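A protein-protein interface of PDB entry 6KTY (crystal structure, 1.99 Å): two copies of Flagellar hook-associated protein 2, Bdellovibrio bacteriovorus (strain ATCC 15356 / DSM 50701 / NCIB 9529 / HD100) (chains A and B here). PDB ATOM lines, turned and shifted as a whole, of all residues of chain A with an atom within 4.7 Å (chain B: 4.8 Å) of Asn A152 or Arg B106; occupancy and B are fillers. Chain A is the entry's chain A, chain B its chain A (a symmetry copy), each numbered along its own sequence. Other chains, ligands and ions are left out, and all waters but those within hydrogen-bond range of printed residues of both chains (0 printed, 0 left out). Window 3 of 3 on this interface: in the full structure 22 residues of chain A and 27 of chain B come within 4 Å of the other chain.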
ATOM      1  N   GLN A  39     -12.313   4.908 -30.819  1.00  0.00           N
ATOM      2  CA  GLN A  39     -13.473   5.435 -30.088  1.00  0.00           C
ATOM      3  C   GLN A  39     -13.335   5.018 -28.643  1.00  0.00           C
ATOM      4  O   GLN A  39     -12.931   3.874 -28.371  1.00  0.00           O
ATOM      5  CB  GLN A  39     -14.699   4.802 -30.741  1.00  0.00           C
ATOM      6  CG  GLN A  39     -16.006   4.974 -30.060  1.00  0.00           C
ATOM      7  CD  GLN A  39     -17.048   4.105 -30.744  1.00  0.00           C
ATOM      8  OE1 GLN A  39     -17.479   4.413 -31.851  1.00  0.00           O
ATOM      9  NE2 GLN A  39     -17.444   3.003 -30.087  1.00  0.00           N
ATOM     10  N   LEU A  40     -13.648   5.909 -27.709  1.00  0.00           N
ATOM     11  CA  LEU A  40     -13.676   5.510 -26.321  1.00  0.00           C
ATOM     12  C   LEU A  40     -14.871   4.579 -26.097  1.00  0.00           C
ATOM     13  O   LEU A  40     -15.849   4.611 -26.837  1.00  0.00           O
ATOM     14  CB  LEU A  40     -13.784   6.715 -25.397  1.00  0.00           C
ATOM     15  CG  LEU A  40     -12.593   7.672 -25.396  1.00  0.00           C
ATOM     16  CD1 LEU A  40     -12.979   8.874 -24.545  1.00  0.00           C
ATOM     17  CD2 LEU A  40     -11.287   7.050 -24.857  1.00  0.00           C
ATOM     18  N   ALA A  41     -14.785   3.741 -25.082  1.00  0.00           N
ATOM     19  CA  ALA A  41     -15.975   3.015 -24.632  1.00  0.00           C
ATOM     20  C   ALA A  41     -17.036   4.026 -24.130  1.00  0.00           C
ATOM     21  O   ALA A  41     -16.675   5.034 -23.542  1.00  0.00           O
ATOM     22  CB  ALA A  41     -15.600   2.037 -23.541  1.00  0.00           C
ATOM     23  N   GLY A 123     -19.368  -0.185 -22.335  1.00  0.00           N
ATOM     24  CA  GLY A 123     -19.296  -1.492 -22.984  1.00  0.00           C
ATOM     25  C   GLY A 123     -20.647  -2.017 -23.425  1.00  0.00           C
ATOM     26  O   GLY A 123     -21.672  -1.746 -22.797  1.00  0.00           O
ATOM     27  N   ASN A 124     -20.669  -2.769 -24.512  1.00  0.00           N
ATOM     28  CA  ASN A 124     -21.922  -3.385 -24.969  1.00  0.00           C
ATOM     29  C   ASN A 124     -22.676  -4.206 -23.954  1.00  0.00           C
ATOM     30  O   ASN A 124     -23.907  -4.244 -23.962  1.00  0.00           O
ATOM     31  CB  ASN A 124     -21.692  -4.265 -26.175  1.00  0.00           C
ATOM     32  CG  ASN A 124     -22.105  -3.582 -27.400  1.00  0.00           C
ATOM     33  OD1 ASN A 124     -21.368  -2.737 -27.919  1.00  0.00           O
ATOM     34  ND2 ASN A 124     -23.330  -3.858 -27.841  1.00  0.00           N
ATOM     35  N   ALA A 150     -24.896   1.915 -24.723  1.00  0.00           N
ATOM     36  CA  ALA A 150     -23.544   1.595 -24.256  1.00  0.00           C
ATOM     37  C   ALA A 150     -22.751   1.023 -25.437  1.00  0.00           C
ATOM     38  O   ALA A 150     -23.301   0.271 -26.263  1.00  0.00           O
ATOM     39  CB  ALA A 150     -23.594   0.571 -23.153  1.00  0.00           C
ATOM     40  N   GLN A 151     -21.473   1.360 -25.501  1.00  0.00           N
ATOM     41  CA  GLN A 151     -20.603   0.824 -26.552  1.00  0.00           C
ATOM     42  C   GLN A 151     -19.220   0.459 -26.056  1.00  0.00           C
ATOM     43  O   GLN A 151     -18.677   1.048 -25.112  1.00  0.00           O
ATOM     44  CB  GLN A 151     -20.393   1.823 -27.677  1.00  0.00           C
ATOM     45  CG  GLN A 151     -21.636   2.285 -28.450  1.00  0.00           C
ATOM     46  CD  GLN A 151     -21.222   3.077 -29.681  1.00  0.00           C
ATOM     47  OE1 GLN A 151     -20.392   2.606 -30.469  1.00  0.00           O
ATOM     48  NE2 GLN A 151     -21.768   4.280 -29.846  1.00  0.00           N
ATOM     49  N   ASN A 152     -18.637  -0.514 -26.754  1.00  0.00           N
ATOM     50  CA  ASN A 152     -17.263  -0.873 -26.571  1.00  0.00           C
ATOM     51  C   ASN A 152     -16.339   0.243 -27.103  1.00  0.00           C
ATOM     52  O   ASN A 152     -16.687   0.990 -28.031  1.00  0.00           O
ATOM     53  CB  ASN A 152     -16.965  -2.205 -27.320  1.00  0.00           C
ATOM     54  CG  ASN A 152     -17.724  -3.391 -26.762  1.00  0.00           C
ATOM     55  OD1 ASN A 152     -18.105  -3.423 -25.578  1.00  0.00           O
ATOM     56  ND2 ASN A 152     -17.929  -4.395 -27.609  1.00  0.00           N
ATOM     57  N   ALA A 153     -15.154   0.343 -26.497  1.00  0.00           N
ATOM     58  CA  ALA A 153     -14.022   1.012 -27.129  1.00  0.00           C
ATOM     59  C   ALA A 153     -13.622   0.284 -28.397  1.00  0.00           C
ATOM     60  O   ALA A 153     -13.782  -0.950 -28.537  1.00  0.00           O
ATOM     61  CB  ALA A 153     -12.847   1.101 -26.207  1.00  0.00           C
ATOM     62  N   LYS A 154     -13.131   1.060 -29.353  1.00  0.00           N
ATOM     63  CA  LYS A 154     -12.559   0.500 -30.560  1.00  0.00           C
ATOM     64  C   LYS A 154     -11.131   0.973 -30.583  1.00  0.00           C
ATOM     65  O   LYS A 154     -10.871   2.183 -30.507  1.00  0.00           O
ATOM     66  CB  LYS A 154     -13.297   0.969 -31.811  1.00  0.00           C
ATOM     67  CG  LYS A 154     -14.734   0.457 -31.930  1.00  0.00           C
ATOM     68  CD  LYS A 154     -15.435   1.069 -33.118  1.00  0.00           C
ATOM     69  CE  LYS A 154     -16.828   0.487 -33.326  1.00  0.00           C
ATOM     70  NZ  LYS A 154     -17.511   1.248 -34.448  1.00  0.00           N
ATOM     71  N   GLU A 163     -12.390  -4.650 -30.155  1.00  0.00           N
ATOM     72  CA  GLU A 163     -13.281  -3.995 -29.230  1.00  0.00           C
ATOM     73  C   GLU A 163     -12.974  -4.376 -27.790  1.00  0.00           C
ATOM     74  O   GLU A 163     -12.746  -5.568 -27.462  1.00  0.00           O
ATOM     75  CB  GLU A 163     -14.750  -4.322 -29.588  1.00  0.00           C
ATOM     76  CG  GLU A 163     -15.156  -3.607 -30.842  1.00  0.00           C
ATOM     77  CD  GLU A 163     -16.618  -3.759 -31.240  1.00  0.00           C
ATOM     78  OE1 GLU A 163     -17.467  -4.175 -30.432  1.00  0.00           O
ATOM     79  OE2 GLU A 163     -16.912  -3.409 -32.396  1.00  0.00           O
ATOM     80  N   LEU A 164     -12.990  -3.366 -26.933  1.00  0.00           N
ATOM     81  CA  LEU A 164     -12.784  -3.536 -25.502  1.00  0.00           C
ATOM     82  C   LEU A 164     -14.002  -2.983 -24.724  1.00  0.00           C
ATOM     83  O   LEU A 164     -14.619  -1.993 -25.118  1.00  0.00           O
ATOM     84  CB  LEU A 164     -11.513  -2.839 -25.045  1.00  0.00           C
ATOM     85  CG  LEU A 164     -10.237  -3.124 -25.860  1.00  0.00           C
ATOM     86  CD1 LEU A 164      -9.090  -2.384 -25.248  1.00  0.00           C
ATOM     87  CD2 LEU A 164      -9.940  -4.597 -25.882  1.00  0.00           C
ATOM     88  N   PRO A 165     -14.339  -3.624 -23.608  1.00  0.00           N
ATOM     89  CA  PRO A 165     -15.466  -3.181 -22.794  1.00  0.00           C
ATOM     90  C   PRO A 165     -15.261  -1.842 -22.062  1.00  0.00           C
ATOM     91  O   PRO A 165     -16.231  -1.084 -21.878  1.00  0.00           O
ATOM     92  CB  PRO A 165     -15.645  -4.341 -21.785  1.00  0.00           C
ATOM     93  CG  PRO A 165     -14.321  -4.993 -21.712  1.00  0.00           C
ATOM     94  CD  PRO A 165     -13.706  -4.859 -23.077  1.00  0.00           C
ATOM     95  N   GLU B 104      -8.009  -9.928 -26.496  1.00  0.00           N
ATOM     96  CA  GLU B 104      -9.430 -10.135 -26.316  1.00  0.00           C
ATOM     97  C   GLU B 104     -10.187  -9.094 -27.142  1.00  0.00           C
ATOM     98  O   GLU B 104      -9.966  -7.889 -26.989  1.00  0.00           O
ATOM     99  CB  GLU B 104      -9.795 -10.007 -24.840  1.00  0.00           C
ATOM    100  CG  GLU B 104     -11.115 -10.637 -24.535  1.00  0.00           C
ATOM    101  CD  GLU B 104     -11.372 -10.853 -23.055  1.00  0.00           C
ATOM    102  OE1 GLU B 104     -12.484 -11.337 -22.739  1.00  0.00           O
ATOM    103  OE2 GLU B 104     -10.471 -10.563 -22.232  1.00  0.00           O
ATOM    104  N   ASP B 105     -11.045  -9.562 -28.039  1.00  0.00           N
ATOM    105  CA  ASP B 105     -11.814  -8.704 -28.916  1.00  0.00           C
ATOM    106  C   ASP B 105     -13.283  -9.001 -28.738  1.00  0.00           C
ATOM    107  O   ASP B 105     -13.782 -10.037 -29.195  1.00  0.00           O
ATOM    108  CB  ASP B 105     -11.411  -8.923 -30.372  1.00  0.00           C
ATOM    109  CG  ASP B 105     -12.266  -8.114 -31.372  1.00  0.00           C
ATOM    110  OD1 ASP B 105     -13.038  -7.210 -30.991  1.00  0.00           O
ATOM    111  OD2 ASP B 105     -12.162  -8.417 -32.566  1.00  0.00           O
ATOM    112  N   ARG B 106     -13.988  -8.064 -28.109  1.00  0.00           N
ATOM    113  CA  ARG B 106     -15.420  -8.232 -27.796  1.00  0.00           C
ATOM    114  C   ARG B 106     -16.397  -8.089 -28.969  1.00  0.00           C
ATOM    115  O   ARG B 106     -17.615  -8.132 -28.759  1.00  0.00           O
ATOM    116  CB  ARG B 106     -15.841  -7.232 -26.720  1.00  0.00           C
ATOM    117  CG  ARG B 106     -15.068  -7.339 -25.430  1.00  0.00           C
ATOM    118  CD  ARG B 106     -14.989  -8.761 -24.939  1.00  0.00           C
ATOM    119  NE  ARG B 106     -14.696  -8.852 -23.510  1.00  0.00           N
ATOM    120  CZ  ARG B 106     -15.579  -8.620 -22.532  1.00  0.00           C
ATOM    121  NH1 ARG B 106     -16.832  -8.250 -22.803  1.00  0.00           N
ATOM    122  NH2 ARG B 106     -15.201  -8.733 -21.263  1.00  0.00           N
ATOM    123  N   LYS B 107     -15.888  -7.936 -30.186  1.00  0.00           N
ATOM    124  CA  LYS B 107     -16.726  -7.978 -31.395  1.00  0.00           C
ATOM    125  C   LYS B 107     -17.596  -9.249 -31.408  1.00  0.00           C
ATOM    126  O   LYS B 107     -18.765  -9.204 -31.767  1.00  0.00           O
ATOM    127  CB  LYS B 107     -15.824  -7.928 -32.645  1.00  0.00           C
ATOM    128  CG  LYS B 107     -16.484  -7.344 -33.883  1.00  0.00           C
ATOM    129  CD  LYS B 107     -15.442  -7.128 -34.981  1.00  0.00           C
ATOM    130  N   ASP B 108     -17.000 -10.383 -31.020  1.00  0.00           N
ATOM    131  CA  ASP B 108     -17.741 -11.638 -30.791  1.00  0.00           C
ATOM    132  C   ASP B 108     -17.575 -12.004 -29.318  1.00  0.00           C
ATOM    133  O   ASP B 108     -16.530 -12.546 -28.925  1.00  0.00           O
ATOM    134  CB  ASP B 108     -17.188 -12.739 -31.705  1.00  0.00           C
ATOM    135  CG  ASP B 108     -17.957 -14.058 -31.594  1.00  0.00           C
ATOM    136  OD1 ASP B 108     -18.763 -14.247 -30.641  1.00  0.00           O
ATOM    137  OD2 ASP B 108     -17.732 -14.906 -32.485  1.00  0.00           O
ATOM    138  N   GLN B 109     -18.595 -11.685 -28.516  1.00  0.00           N
ATOM    139  CA  GLN B 109     -18.555 -11.834 -27.043  1.00  0.00           C
ATOM    140  C   GLN B 109     -18.373 -13.291 -26.629  1.00  0.00           C
ATOM    141  O   GLN B 109     -17.702 -13.577 -25.635  1.00  0.00           O
ATOM    142  CB  GLN B 109     -19.836 -11.253 -26.379  1.00  0.00           C
ATOM    143  CG  GLN B 109     -19.592 -10.431 -25.088  1.00  0.00           C
ATOM    144  CD  GLN B 109     -19.850  -8.921 -25.254  1.00  0.00           C
ATOM    145  OE1 GLN B 109     -19.008  -8.081 -24.897  1.00  0.00           O
ATOM    146  NE2 GLN B 109     -21.040  -8.571 -25.768  1.00  0.00           N
ATOM    147  N   PRO B 112     -14.072 -14.278 -27.808  1.00  0.00           N
ATOM    148  CA  PRO B 112     -13.340 -13.038 -27.759  1.00  0.00           C
ATOM    149  C   PRO B 112     -11.822 -13.195 -27.955  1.00  0.00           C
ATOM    150  O   PRO B 112     -11.164 -12.228 -28.363  1.00  0.00           O
ATOM    151  CB  PRO B 112     -13.673 -12.514 -26.362  1.00  0.00           C
ATOM    152  CG  PRO B 112     -13.851 -13.706 -25.535  1.00  0.00           C
ATOM    153  CD  PRO B 112     -14.304 -14.820 -26.463  1.00  0.00           C
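The backbone NH (N) of Glu A163 lies within hydrogen-bond range of the side-chain carboxylate (OD1) of Asp B105 (2.8 Å). O of Glu A163 is in hydrogen-bond range of N of Arg B106, 2.9 Å away.
The backbone carbonyl oxygen (O) of Pro B112 sits at hydrogen-bond distance from the backbone NH (N) of Asp B105. The backbone NH of Ala A153 is in hydrogen-bond range of the backbone carbonyl oxygen of Leu A164 (2.8 Å). The side-chain carboxylate (OD1) of Asp B105 lies within hydrogen-bond range of the backbone NH (N) of Lys B107 (3.0 Å). The side-chain carboxylate (OE1) of Glu A163 is in hydrogen-bond range of the side-chain amide nitrogen (ND2) of Asn A152 (2.9 Å). The backbone NH of Gly A123 lies close to the backbone carbonyl oxygen of Pro A165 (3.3 Å). The side-chain amide oxygen of Asn A152 sits at hydrogen-bond distance from the backbone NH of Asn A124 (2.9 Å).
Among the printed residues, pairs that only touch across the chains: Asn A152 with Arg B106 (3.6 Å), Glu A163 with Glu B104 (3.7 Å), Glu A163 with Lys B107 (3.8 Å), Leu A164 with Glu B104 (3.5 Å) and Pro A165 with Arg B106 (3.7 Å).
Asn A152 touches just one residue of chain B: Arg B106 (3.6 Å). Of chain A, only Asn A152 (3.6 Å), Glu A163 (2.9 Å) and Pro A165 (3.7 Å) come within 4 Å of Arg B106. Of the printed residues of chain B, Pro A165 touches Arg B106. Of the printed residues of chain B, Leu A164 touches Glu B104 (3.5 Å). Printed residues of chain A within 4 Å of Lys B107: Glu A163 (3.8 Å). Of the printed residues of chain A, Asp B105 touches Glu A163 (2.8 Å). The nearest residue of chain B that does not touch Asn A152 is Gln B109 (4.7 Å). The nearest residue of chain A that does not touch Arg B106 is Leu A164 (4.4 Å). The nearest printed residue of chain B that does not touch Glu A163 is Asp B108 (6.3 Å).
Hydrophobic or aromatic side chains of chain A within 4 Å of the printed part of chain B: Leu A164 and Pro A165. Of the 7 printed residues of chain B, 4 touch a printed residue of chain A.
No position is printed for both chains.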
